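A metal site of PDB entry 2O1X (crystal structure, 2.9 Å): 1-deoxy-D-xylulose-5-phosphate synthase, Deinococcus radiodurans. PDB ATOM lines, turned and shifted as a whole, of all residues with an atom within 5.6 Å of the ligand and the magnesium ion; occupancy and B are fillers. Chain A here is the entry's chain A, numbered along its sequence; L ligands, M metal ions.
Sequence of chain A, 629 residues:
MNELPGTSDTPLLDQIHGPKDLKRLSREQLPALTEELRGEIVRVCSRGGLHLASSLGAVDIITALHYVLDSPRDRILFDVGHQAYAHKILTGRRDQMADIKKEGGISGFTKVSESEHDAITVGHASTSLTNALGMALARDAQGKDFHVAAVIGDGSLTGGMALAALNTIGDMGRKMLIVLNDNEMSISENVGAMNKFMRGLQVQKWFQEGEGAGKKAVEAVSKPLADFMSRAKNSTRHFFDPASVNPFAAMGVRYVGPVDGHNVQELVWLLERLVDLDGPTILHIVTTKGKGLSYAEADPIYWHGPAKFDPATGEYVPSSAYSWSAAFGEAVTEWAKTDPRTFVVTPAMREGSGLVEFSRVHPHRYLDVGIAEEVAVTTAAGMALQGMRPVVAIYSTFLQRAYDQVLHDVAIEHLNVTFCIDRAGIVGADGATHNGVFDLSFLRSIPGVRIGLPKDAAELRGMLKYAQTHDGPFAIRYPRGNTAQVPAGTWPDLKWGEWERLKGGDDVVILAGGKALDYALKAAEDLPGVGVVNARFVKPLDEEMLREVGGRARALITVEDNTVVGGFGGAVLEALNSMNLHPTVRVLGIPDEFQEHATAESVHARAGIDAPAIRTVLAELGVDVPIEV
The backbone carbonyl oxygen of Ser 186 lies close to an oxygen (O5) of the ligand, 3.1 Å away. CG1 of Val 80 touches N3 of the ligand, at 3.9 Å. His 124 touches the ligand (CA to N2, 3.5 Å). Gly 153 touches the ligand (CA to O3, 3.2 Å). CG1 of Ile 187 touches C8 of the ligand, at 3.5 Å. His 304 touches the ligand. CB of Ala 348 touches C10 of the ligand (3.9 Å). Met 349 touches the ligand (CE to C10, 3.6 Å). Ile 371 touches the ligand (CD1 to C10, 3.3 Å). CD1 of Phe 398 touches C1 of the ligand, 3.3 Å away. NH1 of Arg 401 touches C2 of the ligand, at 3.7 Å. Hydrophobic or aromatic side chains that line the ligand: Val 80, His 82, Ala 125, Ile 187, His 304, Ala 348, Met 349, Ile 371 and Phe 398. Of the 32 residues printed, 22 come within 4 Å of the ligand. The nearest printed residue that does not touch the ligand is Asn 181 (4.4 Å).
OE2 of Glu 373 is in hydrogen-bond range of N1 of the ligand, at 2.7 Å. N of Gly 155 sits close to O2 of the ligand (2.9 Å). The backbone NH of Asp 154 sits close to an oxygen (O2) of the ligand (3.2 Å). The side-chain amino group (NZ) of Lys 289 lies within salt-bridge range of an oxygen (O5) of the ligand, at 3.8 Å. N of Ser 156 sits at hydrogen-bond distance from O3 of the ligand (3.3 Å). O of Gly 123 sits at hydrogen-bond distance from N3 of the ligand (2.9 Å). The side-chain hydroxyl of Ser 156 lies within hydrogen-bond range of an oxygen (O3) of the ligand, at 3.4 Å. OG of Ser 54 sits at hydrogen-bond distance from O5 of the ligand (2.9 Å). N of Ala 125 sits at hydrogen-bond distance from N2 of the ligand (3.1 Å). An oxygen (O4) of the ligand sits at hydrogen-bond distance from a ring nitrogen (NE2) of His 82, 3.4 Å away.
The side-chain carboxylate (OD1) of Asp 79 lies within hydrogen-bond range of the side-chain hydroxyl (OG) of Ser 156 (2.5 Å). The side-chain amide oxygen (OD1) of Asn 190 lies close to the side-chain carboxylate (OD1) of Asp 154 (2.9 Å). The backbone NH of Asp 154 lies within hydrogen-bond range of the backbone carbonyl oxygen of Asn 181 (3.4 Å). OD1 of Asp 154 lies close to N of Glu 184, at 3.4 Å. N of Gly 155 lies within hydrogen-bond range of OD1 of Asn 190. The side-chain amino group (NZ) of Lys 289 sits at hydrogen-bond distance from the backbone carbonyl oxygen (O) of Ser 186. O of Ala 125 lies within hydrogen-bond range of NH2 of Arg 401 (2.7 Å). The backbone NH (N) of Gly 123 is in hydrogen-bond range of the backbone carbonyl oxygen (O) of Val 80, 3.4 Å away.
The magnesium ion is bound by an oxygen (O6) of the ligand (1.9 Å), the side-chain amide nitrogen (ND2) of Asn 183 (2.1 Å), the side-chain carboxylate (OD2) of Asp 154 (2.1 Å), an oxygen (O2) of the ligand (2.2 Å) and the backbone carbonyl oxygen (O) of Met 185 (2.5 Å). The magnesium ion has five donor atoms within binding distance.
Merely in contact with the magnesium ion: Asn 181 (3.5 Å). Four residues have an atom within 4 Å of the magnesium ion: Asp 154, Asn 181, Asn 183 and Met 185. The nearest printed residue that does not touch the magnesium ion is Gly 153 (4.3 Å).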
ATOM      1  N   SER A  54       7.614   6.793  -6.417  1.00  0.00           N
ATOM      2  CA  SER A  54       7.535   5.353  -6.460  1.00  0.00           C
ATOM      3  C   SER A  54       7.539   4.861  -7.894  1.00  0.00           C
ATOM      4  O   SER A  54       8.096   3.807  -8.184  1.00  0.00           O
ATOM      5  CB  SER A  54       6.259   4.882  -5.769  1.00  0.00           C
ATOM      6  OG  SER A  54       6.422   4.865  -4.361  1.00  0.00           O
ATOM      7  N   ASP A  79       2.154  -4.993  -6.552  1.00  0.00           N
ATOM      8  CA  ASP A  79       1.715  -4.741  -5.187  1.00  0.00           C
ATOM      9  C   ASP A  79       1.464  -3.247  -4.946  1.00  0.00           C
ATOM     10  O   ASP A  79       2.330  -2.411  -5.246  1.00  0.00           O
ATOM     11  CB  ASP A  79       2.726  -5.305  -4.195  1.00  0.00           C
ATOM     12  CG  ASP A  79       2.137  -5.538  -2.830  1.00  0.00           C
ATOM     13  OD1 ASP A  79       2.092  -4.568  -2.041  1.00  0.00           O
ATOM     14  OD2 ASP A  79       1.695  -6.644  -2.440  1.00  0.00           O
ATOM     15  N   VAL A  80       0.286  -2.925  -4.394  1.00  0.00           N
ATOM     16  CA  VAL A  80      -0.283  -1.561  -4.258  1.00  0.00           C
ATOM     17  C   VAL A  80      -0.675  -0.923  -5.607  1.00  0.00           C
ATOM     18  O   VAL A  80      -1.831  -0.549  -5.810  1.00  0.00           O
ATOM     19  CB  VAL A  80       0.575  -0.563  -3.427  1.00  0.00           C
ATOM     20  CG1 VAL A  80      -0.258   0.658  -3.045  1.00  0.00           C
ATOM     21  CG2 VAL A  80       1.101  -1.219  -2.187  1.00  0.00           C
ATOM     22  N   HIS A  82       0.799   1.767  -7.018  1.00  0.00           N
ATOM     23  CA  HIS A  82       1.179   3.182  -7.083  1.00  0.00           C
ATOM     24  C   HIS A  82       2.492   3.357  -7.838  1.00  0.00           C
ATOM     25  O   HIS A  82       2.870   4.470  -8.175  1.00  0.00           O
ATOM     26  CB  HIS A  82       1.314   3.748  -5.671  1.00  0.00           C
ATOM     27  CG  HIS A  82       2.425   3.130  -4.888  1.00  0.00           C
ATOM     28  ND1 HIS A  82       2.550   1.759  -4.734  1.00  0.00           N
ATOM     29  CD2 HIS A  82       3.472   3.680  -4.219  1.00  0.00           C
ATOM     30  CE1 HIS A  82       3.622   1.501  -4.005  1.00  0.00           C
ATOM     31  NE2 HIS A  82       4.194   2.644  -3.689  1.00  0.00           N
ATOM     32  N   GLN A  83       3.193   2.248  -8.114  1.00  0.00           N
ATOM     33  CA  GLN A  83       4.480   2.352  -8.763  1.00  0.00           C
ATOM     34  C   GLN A  83       4.440   2.036 -10.250  1.00  0.00           C
ATOM     35  O   GLN A  83       5.493   1.995 -10.899  1.00  0.00           O
ATOM     36  CB  GLN A  83       5.493   1.431  -8.082  1.00  0.00           C
ATOM     37  CG  GLN A  83       5.392  -0.048  -8.454  1.00  0.00           C
ATOM     38  CD  GLN A  83       4.500  -0.837  -7.502  1.00  0.00           C
ATOM     39  OE1 GLN A  83       3.282  -0.736  -7.539  1.00  0.00           O
ATOM     40  NE2 GLN A  83       5.122  -1.658  -6.658  1.00  0.00           N
ATOM     41  N   GLY A 123      -4.692  -1.473  -4.198  1.00  0.00           N
ATOM     42  CA  GLY A 123      -4.863  -0.207  -3.504  1.00  0.00           C
ATOM     43  C   GLY A 123      -4.304  -0.432  -2.114  1.00  0.00           C
ATOM     44  O   GLY A 123      -3.443   0.318  -1.680  1.00  0.00           O
ATOM     45  N   HIS A 124      -4.798  -1.475  -1.448  1.00  0.00           N
ATOM     46  CA  HIS A 124      -4.220  -1.986  -0.210  1.00  0.00           C
ATOM     47  C   HIS A 124      -2.932  -2.745  -0.542  1.00  0.00           C
ATOM     48  O   HIS A 124      -2.808  -3.349  -1.603  1.00  0.00           O
ATOM     49  CB  HIS A 124      -5.208  -2.906   0.487  1.00  0.00           C
ATOM     50  CG  HIS A 124      -6.369  -2.190   1.118  1.00  0.00           C
ATOM     51  ND1 HIS A 124      -7.236  -2.811   2.000  1.00  0.00           N
ATOM     52  CD2 HIS A 124      -6.780  -0.905   1.017  1.00  0.00           C
ATOM     53  CE1 HIS A 124      -8.142  -1.941   2.405  1.00  0.00           C
ATOM     54  NE2 HIS A 124      -7.889  -0.771   1.834  1.00  0.00           N
ATOM     55  N   ALA A 125      -1.953  -2.698   0.363  1.00  0.00           N
ATOM     56  CA  ALA A 125      -0.641  -3.300   0.117  1.00  0.00           C
ATOM     57  C   ALA A 125      -0.659  -4.792   0.376  1.00  0.00           C
ATOM     58  O   ALA A 125      -1.642  -5.326   0.913  1.00  0.00           O
ATOM     59  CB  ALA A 125       0.378  -2.643   1.011  1.00  0.00           C
ATOM     60  N   ILE A 152       6.717  -6.590  -5.700  1.00  0.00           N
ATOM     61  CA  ILE A 152       6.461  -6.106  -4.339  1.00  0.00           C
ATOM     62  C   ILE A 152       7.614  -5.228  -3.789  1.00  0.00           C
ATOM     63  O   ILE A 152       8.794  -5.628  -3.814  1.00  0.00           O
ATOM     64  CB  ILE A 152       6.117  -7.285  -3.383  1.00  0.00           C
ATOM     65  CG1 ILE A 152       5.610  -6.761  -2.041  1.00  0.00           C
ATOM     66  CG2 ILE A 152       7.306  -8.231  -3.169  1.00  0.00           C
ATOM     67  CD1 ILE A 152       4.631  -7.692  -1.364  1.00  0.00           C
ATOM     68  N   GLY A 153       7.259  -4.040  -3.319  1.00  0.00           N
ATOM     69  CA  GLY A 153       8.209  -3.169  -2.646  1.00  0.00           C
ATOM     70  C   GLY A 153       8.523  -3.696  -1.246  1.00  0.00           C
ATOM     71  O   GLY A 153       7.899  -4.662  -0.777  1.00  0.00           O
ATOM     72  N   ASP A 154       9.480  -3.063  -0.566  1.00  0.00           N
ATOM     73  CA  ASP A 154      10.019  -3.614   0.662  1.00  0.00           C
ATOM     74  C   ASP A 154       9.143  -3.331   1.889  1.00  0.00           C
ATOM     75  O   ASP A 154       9.061  -4.153   2.806  1.00  0.00           O
ATOM     76  CB  ASP A 154      11.456  -3.152   0.860  1.00  0.00           C
ATOM     77  CG  ASP A 154      11.584  -1.654   1.024  1.00  0.00           C
ATOM     78  OD1 ASP A 154      12.095  -1.259   2.101  1.00  0.00           O
ATOM     79  OD2 ASP A 154      11.223  -0.808   0.176  1.00  0.00           O
ATOM     80  N   GLY A 155       8.468  -2.181   1.892  1.00  0.00           N
ATOM     81  CA  GLY A 155       7.470  -1.866   2.913  1.00  0.00           C
ATOM     82  C   GLY A 155       6.284  -2.813   2.820  1.00  0.00           C
ATOM     83  O   GLY A 155       5.741  -3.260   3.826  1.00  0.00           O
ATOM     84  N   SER A 156       5.888  -3.138   1.594  1.00  0.00           N
ATOM     85  CA  SER A 156       4.777  -4.057   1.358  1.00  0.00           C
ATOM     86  C   SER A 156       4.999  -5.436   1.960  1.00  0.00           C
ATOM     87  O   SER A 156       4.075  -6.040   2.524  1.00  0.00           O
ATOM     88  CB  SER A 156       4.525  -4.165  -0.123  1.00  0.00           C
ATOM     89  OG  SER A 156       3.472  -3.307  -0.449  1.00  0.00           O
ATOM     90  N   LEU A 157       6.237  -5.896   1.819  1.00  0.00           N
ATOM     91  CA  LEU A 157       6.726  -7.160   2.381  1.00  0.00           C
ATOM     92  C   LEU A 157       6.598  -7.205   3.916  1.00  0.00           C
ATOM     93  O   LEU A 157       6.613  -8.282   4.510  1.00  0.00           O
ATOM     94  CB  LEU A 157       8.182  -7.372   1.963  1.00  0.00           C
ATOM     95  CG  LEU A 157       8.856  -8.732   2.177  1.00  0.00           C
ATOM     96  CD1 LEU A 157       8.251  -9.817   1.283  1.00  0.00           C
ATOM     97  CD2 LEU A 157      10.359  -8.590   1.955  1.00  0.00           C
ATOM     98  N   ASN A 181      11.150  -5.122  -4.864  1.00  0.00           N
ATOM     99  CA  ASN A 181      11.573  -3.761  -5.170  1.00  0.00           C
ATOM    100  C   ASN A 181      12.034  -3.001  -3.934  1.00  0.00           C
ATOM    101  O   ASN A 181      11.268  -2.231  -3.346  1.00  0.00           O
ATOM    102  CB  ASN A 181      10.434  -3.005  -5.848  1.00  0.00           C
ATOM    103  CG  ASN A 181      10.835  -1.604  -6.248  1.00  0.00           C
ATOM    104  OD1 ASN A 181      12.009  -1.294  -6.335  1.00  0.00           O
ATOM    105  ND2 ASN A 181       9.862  -0.755  -6.482  1.00  0.00           N
ATOM    106  N   ASP A 182      13.291  -3.210  -3.537  1.00  0.00           N
ATOM    107  CA  ASP A 182      13.771  -2.714  -2.243  1.00  0.00           C
ATOM    108  C   ASP A 182      14.493  -1.375  -2.334  1.00  0.00           C
ATOM    109  O   ASP A 182      15.667  -1.322  -2.661  1.00  0.00           O
ATOM    110  CB  ASP A 182      14.639  -3.791  -1.546  1.00  0.00           C
ATOM    111  CG  ASP A 182      15.275  -3.310  -0.219  1.00  0.00           C
ATOM    112  OD1 ASP A 182      16.376  -3.813   0.102  1.00  0.00           O
ATOM    113  OD2 ASP A 182      14.776  -2.456   0.549  1.00  0.00           O
ATOM    114  N   ASN A 183      13.782  -0.295  -2.047  1.00  0.00           N
ATOM    115  CA  ASN A 183      14.404   1.023  -1.940  1.00  0.00           C
ATOM    116  C   ASN A 183      14.503   1.537  -0.531  1.00  0.00           C
ATOM    117  O   ASN A 183      14.727   2.705  -0.315  1.00  0.00           O
ATOM    118  CB  ASN A 183      13.686   2.062  -2.787  1.00  0.00           C
ATOM    119  CG  ASN A 183      12.233   2.252  -2.405  1.00  0.00           C
ATOM    120  OD1 ASN A 183      11.510   2.952  -3.109  1.00  0.00           O
ATOM    121  ND2 ASN A 183      11.769   1.635  -1.311  1.00  0.00           N
ATOM    122  N   GLU A 184      14.320   0.629   0.428  1.00  0.00           N
ATOM    123  CA  GLU A 184      14.252   0.939   1.867  1.00  0.00           C
ATOM    124  C   GLU A 184      13.399   2.183   2.241  1.00  0.00           C
ATOM    125  O   GLU A 184      13.616   2.832   3.270  1.00  0.00           O
ATOM    126  CB  GLU A 184      15.628   0.932   2.513  1.00  0.00           C
ATOM    127  CG  GLU A 184      16.534   2.075   2.118  1.00  0.00           C
ATOM    128  CD  GLU A 184      17.956   1.872   2.593  1.00  0.00           C
ATOM    129  OE1 GLU A 184      18.257   0.820   3.187  1.00  0.00           O
ATOM    130  OE2 GLU A 184      18.765   2.777   2.353  1.00  0.00           O
ATOM    131  N   MET A 185      12.431   2.479   1.389  1.00  0.00           N
ATOM    132  CA  MET A 185      11.363   3.388   1.747  1.00  0.00           C
ATOM    133  C   MET A 185      10.028   2.646   1.728  1.00  0.00           C
ATOM    134  O   MET A 185       9.804   1.736   0.889  1.00  0.00           O
ATOM    135  CB  MET A 185      11.318   4.590   0.804  1.00  0.00           C
ATOM    136  CG  MET A 185      12.540   5.472   0.842  1.00  0.00           C
ATOM    137  SD  MET A 185      12.648   6.395   2.373  1.00  0.00           S
ATOM    138  CE  MET A 185      14.373   6.111   2.802  1.00  0.00           C
ATOM    139  N   SER A 186       9.174   3.021   2.699  1.00  0.00           N
ATOM    140  CA  SER A 186       7.727   2.821   2.653  1.00  0.00           C
ATOM    141  C   SER A 186       7.144   4.128   2.106  1.00  0.00           C
ATOM    142  O   SER A 186       7.493   4.558   1.001  1.00  0.00           O
ATOM    143  CB  SER A 186       7.201   2.507   4.051  1.00  0.00           C
ATOM    144  OG  SER A 186       6.058   1.668   4.009  1.00  0.00           O
ATOM    145  N   ILE A 187       6.275   4.794   2.849  1.00  0.00           N
ATOM    146  CA  ILE A 187       5.934   6.175   2.521  1.00  0.00           C
ATOM    147  C   ILE A 187       6.924   6.991   3.356  1.00  0.00           C
ATOM    148  O   ILE A 187       7.678   7.837   2.836  1.00  0.00           O
ATOM    149  CB  ILE A 187       4.446   6.515   2.827  1.00  0.00           C
ATOM    150  CG1 ILE A 187       3.534   5.736   1.879  1.00  0.00           C
ATOM    151  CG2 ILE A 187       4.219   8.022   2.764  1.00  0.00           C
ATOM    152  CD1 ILE A 187       2.100   6.175   1.812  1.00  0.00           C
ATOM    153  N   ASN A 190      11.177   3.015   5.710  1.00  0.00           N
ATOM    154  CA  ASN A 190      10.695   1.680   6.043  1.00  0.00           C
ATOM    155  C   ASN A 190      11.162   1.210   7.415  1.00  0.00           C
ATOM    156  O   ASN A 190      12.274   1.505   7.834  1.00  0.00           O
ATOM    157  CB  ASN A 190      11.082   0.661   4.986  1.00  0.00           C
ATOM    158  CG  ASN A 190      10.206  -0.562   5.000  1.00  0.00           C
ATOM    159  OD1 ASN A 190      10.578  -1.621   4.512  1.00  0.00           O
ATOM    160  ND2 ASN A 190       9.001  -0.421   5.557  1.00  0.00           N
ATOM    161  N   LYS A 289      14.116   5.535  -4.614  1.00  0.00           N
ATOM    162  CA  LYS A 289      12.794   6.173  -4.677  1.00  0.00           C
ATOM    163  C   LYS A 289      13.045   7.556  -5.240  1.00  0.00           C
ATOM    164  O   LYS A 289      13.889   8.317  -4.708  1.00  0.00           O
ATOM    165  CB  LYS A 289      12.099   6.214  -3.298  1.00  0.00           C
ATOM    166  CG  LYS A 289      10.630   6.662  -3.334  1.00  0.00           C
ATOM    167  CD  LYS A 289       9.726   5.655  -2.606  1.00  0.00           C
ATOM    168  CE  LYS A 289       8.413   6.248  -2.117  1.00  0.00           C
ATOM    169  NZ  LYS A 289       8.543   6.821  -0.720  1.00  0.00           N
ATOM    170  N   HIS A 304       6.688  11.310  -2.693  1.00  0.00           N
ATOM    171  CA  HIS A 304       5.860  10.113  -2.813  1.00  0.00           C
ATOM    172  C   HIS A 304       4.502  10.411  -3.473  1.00  0.00           C
ATOM    173  O   HIS A 304       4.047   9.671  -4.361  1.00  0.00           O
ATOM    174  CB  HIS A 304       5.645   9.468  -1.433  1.00  0.00           C
ATOM    175  CG  HIS A 304       4.838   8.210  -1.481  1.00  0.00           C
ATOM    176  ND1 HIS A 304       3.470   8.206  -1.285  1.00  0.00           N
ATOM    177  CD2 HIS A 304       5.191   6.934  -1.741  1.00  0.00           C
ATOM    178  CE1 HIS A 304       3.025   6.964  -1.414  1.00  0.00           C
ATOM    179  NE2 HIS A 304       4.043   6.175  -1.686  1.00  0.00           N
ATOM    180  N   PRO A 347       0.379   2.214  11.661  1.00  0.00           N
ATOM    181  CA  PRO A 347       0.772   1.219  10.685  1.00  0.00           C
ATOM    182  C   PRO A 347       1.255   1.944   9.450  1.00  0.00           C
ATOM    183  O   PRO A 347       0.464   2.169   8.538  1.00  0.00           O
ATOM    184  CB  PRO A 347      -0.529   0.459  10.405  1.00  0.00           C
ATOM    185  CG  PRO A 347      -1.655   1.412  10.777  1.00  0.00           C
ATOM    186  CD  PRO A 347      -1.031   2.600  11.508  1.00  0.00           C
ATOM    187  N   ALA A 348       2.538   2.344   9.466  1.00  0.00           N
ATOM    188  CA  ALA A 348       3.237   2.954   8.310  1.00  0.00           C
ATOM    189  C   ALA A 348       2.781   4.358   7.857  1.00  0.00           C
ATOM    190  O   ALA A 348       3.282   4.867   6.847  1.00  0.00           O
ATOM    191  CB  ALA A 348       3.275   1.991   7.132  1.00  0.00           C
ATOM    192  N   MET A 349       1.854   4.988   8.580  1.00  0.00           N
ATOM    193  CA  MET A 349       1.263   6.249   8.129  1.00  0.00           C
ATOM    194  C   MET A 349       1.493   7.479   9.026  1.00  0.00           C
ATOM    195  O   MET A 349       0.650   8.378   9.091  1.00  0.00           O
ATOM    196  CB  MET A 349      -0.232   6.057   7.831  1.00  0.00           C
ATOM    197  CG  MET A 349      -0.514   5.099   6.707  1.00  0.00           C
ATOM    198  SD  MET A 349      -0.289   5.818   5.074  1.00  0.00           S
ATOM    199  CE  MET A 349       1.409   5.392   4.856  1.00  0.00           C
ATOM    200  N   ILE A 371       3.551  -1.813   7.384  1.00  0.00           N
ATOM    201  CA  ILE A 371       2.238  -1.944   6.747  1.00  0.00           C
ATOM    202  C   ILE A 371       1.527  -3.187   7.270  1.00  0.00           C
ATOM    203  O   ILE A 371       1.221  -4.111   6.517  1.00  0.00           O
ATOM    204  CB  ILE A 371       2.313  -1.941   5.207  1.00  0.00           C
ATOM    205  CG1 ILE A 371       3.444  -1.018   4.735  1.00  0.00           C
ATOM    206  CG2 ILE A 371       0.946  -1.534   4.639  1.00  0.00           C
ATOM    207  CD1 ILE A 371       3.501  -0.734   3.225  1.00  0.00           C
ATOM    208  N   GLU A 373      -1.523  -3.598   9.875  1.00  0.00           N
ATOM    209  CA  GLU A 373      -2.594  -3.035  10.691  1.00  0.00           C
ATOM    210  C   GLU A 373      -2.931  -3.980  11.801  1.00  0.00           C
ATOM    211  O   GLU A 373      -3.163  -3.558  12.932  1.00  0.00           O
ATOM    212  CB  GLU A 373      -3.842  -2.792   9.831  1.00  0.00           C
ATOM    213  CG  GLU A 373      -3.811  -1.514   9.000  1.00  0.00           C
ATOM    214  CD  GLU A 373      -2.924  -1.553   7.755  1.00  0.00           C
ATOM    215  OE1 GLU A 373      -2.320  -2.599   7.431  1.00  0.00           O
ATOM    216  OE2 GLU A 373      -2.817  -0.508   7.080  1.00  0.00           O
ATOM    217  N   PHE A 398      -7.954   1.085   6.021  1.00  0.00           N
ATOM    218  CA  PHE A 398      -6.935   0.140   6.429  1.00  0.00           C
ATOM    219  C   PHE A 398      -7.271  -0.477   7.769  1.00  0.00           C
ATOM    220  O   PHE A 398      -6.763  -1.538   8.125  1.00  0.00           O
ATOM    221  CB  PHE A 398      -5.573   0.822   6.492  1.00  0.00           C
ATOM    222  CG  PHE A 398      -5.170   1.495   5.218  1.00  0.00           C
ATOM    223  CD1 PHE A 398      -5.340   0.859   3.989  1.00  0.00           C
ATOM    224  CD2 PHE A 398      -4.623   2.759   5.236  1.00  0.00           C
ATOM    225  CE1 PHE A 398      -4.984   1.479   2.804  1.00  0.00           C
ATOM    226  CE2 PHE A 398      -4.265   3.384   4.059  1.00  0.00           C
ATOM    227  CZ  PHE A 398      -4.453   2.741   2.841  1.00  0.00           C
ATOM    228  N   ARG A 401      -8.410  -4.027   7.571  1.00  0.00           N
ATOM    229  CA  ARG A 401      -7.432  -5.075   7.750  1.00  0.00           C
ATOM    230  C   ARG A 401      -7.336  -5.633   9.167  1.00  0.00           C
ATOM    231  O   ARG A 401      -6.659  -6.629   9.398  1.00  0.00           O
ATOM    232  CB  ARG A 401      -6.072  -4.598   7.288  1.00  0.00           C
ATOM    233  CG  ARG A 401      -5.914  -4.730   5.811  1.00  0.00           C
ATOM    234  CD  ARG A 401      -5.686  -6.159   5.333  1.00  0.00           C
ATOM    235  NE  ARG A 401      -5.378  -6.185   3.910  1.00  0.00           N
ATOM    236  CZ  ARG A 401      -4.178  -5.935   3.392  1.00  0.00           C
ATOM    237  NH1 ARG A 401      -3.160  -5.671   4.188  1.00  0.00           N
ATOM    238  NH2 ARG A 401      -4.004  -5.943   2.077  1.00  0.00           N
ATOM    239  N   HIS A 434     -10.008   2.639  -1.664  1.00  0.00           N
ATOM    240  CA  HIS A 434      -9.618   3.521  -0.561  1.00  0.00           C
ATOM    241  C   HIS A 434     -10.694   4.239   0.178  1.00  0.00           C
ATOM    242  O   HIS A 434     -10.424   4.747   1.271  1.00  0.00           O
ATOM    243  CB  HIS A 434      -8.616   4.556  -1.040  1.00  0.00           C
ATOM    244  CG  HIS A 434      -7.211   4.072  -0.996  1.00  0.00           C
ATOM    245  ND1 HIS A 434      -6.734   3.113  -1.861  1.00  0.00           N
ATOM    246  CD2 HIS A 434      -6.184   4.404  -0.187  1.00  0.00           C
ATOM    247  CE1 HIS A 434      -5.458   2.890  -1.599  1.00  0.00           C
ATOM    248  NE2 HIS A 434      -5.100   3.654  -0.582  1.00  0.00           N
HETATM  249  N1  LIG L   1      -1.986   0.188   4.572  1.00  0.00           N
HETATM  250  C1  LIG L   1      -2.482  -0.681   3.697  1.00  0.00           C
HETATM  251  C2  LIG L   1      -3.180  -1.946   4.191  1.00  0.00           C
HETATM  252  N2  LIG L   1      -2.378  -0.436   2.372  1.00  0.00           N
HETATM  253  C3  LIG L   1      -1.774   0.662   1.908  1.00  0.00           C
HETATM  254  N3  LIG L   1      -1.699   0.848   0.595  1.00  0.00           N
HETATM  255  C4  LIG L   1      -1.230   1.571   2.815  1.00  0.00           C
HETATM  256  C5  LIG L   1      -1.383   1.277   4.165  1.00  0.00           C
HETATM  257  C6  LIG L   1      -0.528   2.894   2.505  1.00  0.00           C
HETATM  258  N4  LIG L   1       0.574   2.811   1.531  1.00  0.00           N
HETATM  259  C7  LIG L   1       0.351   3.023   0.213  1.00  0.00           C
HETATM  260  S1  LIG L   1       1.922   2.838  -0.586  1.00  0.00           S
HETATM  261  C8  LIG L   1       2.773   2.532   0.848  1.00  0.00           C
HETATM  262  C9  LIG L   1       1.862   2.552   1.901  1.00  0.00           C
HETATM  263  C10 LIG L   1       2.345   2.311   3.327  1.00  0.00           C
HETATM  264  C11 LIG L   1       4.273   2.306   0.875  1.00  0.00           C
HETATM  265  C12 LIG L   1       4.643   1.149  -0.021  1.00  0.00           C
HETATM  266  O1  LIG L   1       5.936   0.775   0.349  1.00  0.00           O
HETATM  267  P1  LIG L   1       6.730  -0.006  -0.716  1.00  0.00           P
HETATM  268  O2  LIG L   1       8.254  -0.149  -0.140  1.00  0.00           O
HETATM  269  O3  LIG L   1       6.100  -1.284  -1.109  1.00  0.00           O
HETATM  270  O4  LIG L   1       6.640   0.952  -2.042  1.00  0.00           O
HETATM  271  P2  LIG L   1       7.635   2.115  -2.543  1.00  0.00           P
HETATM  272  O5  LIG L   1       7.121   3.544  -1.919  1.00  0.00           O
HETATM  273  O6  LIG L   1       9.145   1.792  -1.967  1.00  0.00           O
HETATM  274  O7  LIG L   1       7.638   2.186  -4.004  1.00  0.00           O
HETATM  275 MG    MG M   1      10.166   0.350  -1.188  1.00  0.00          MG
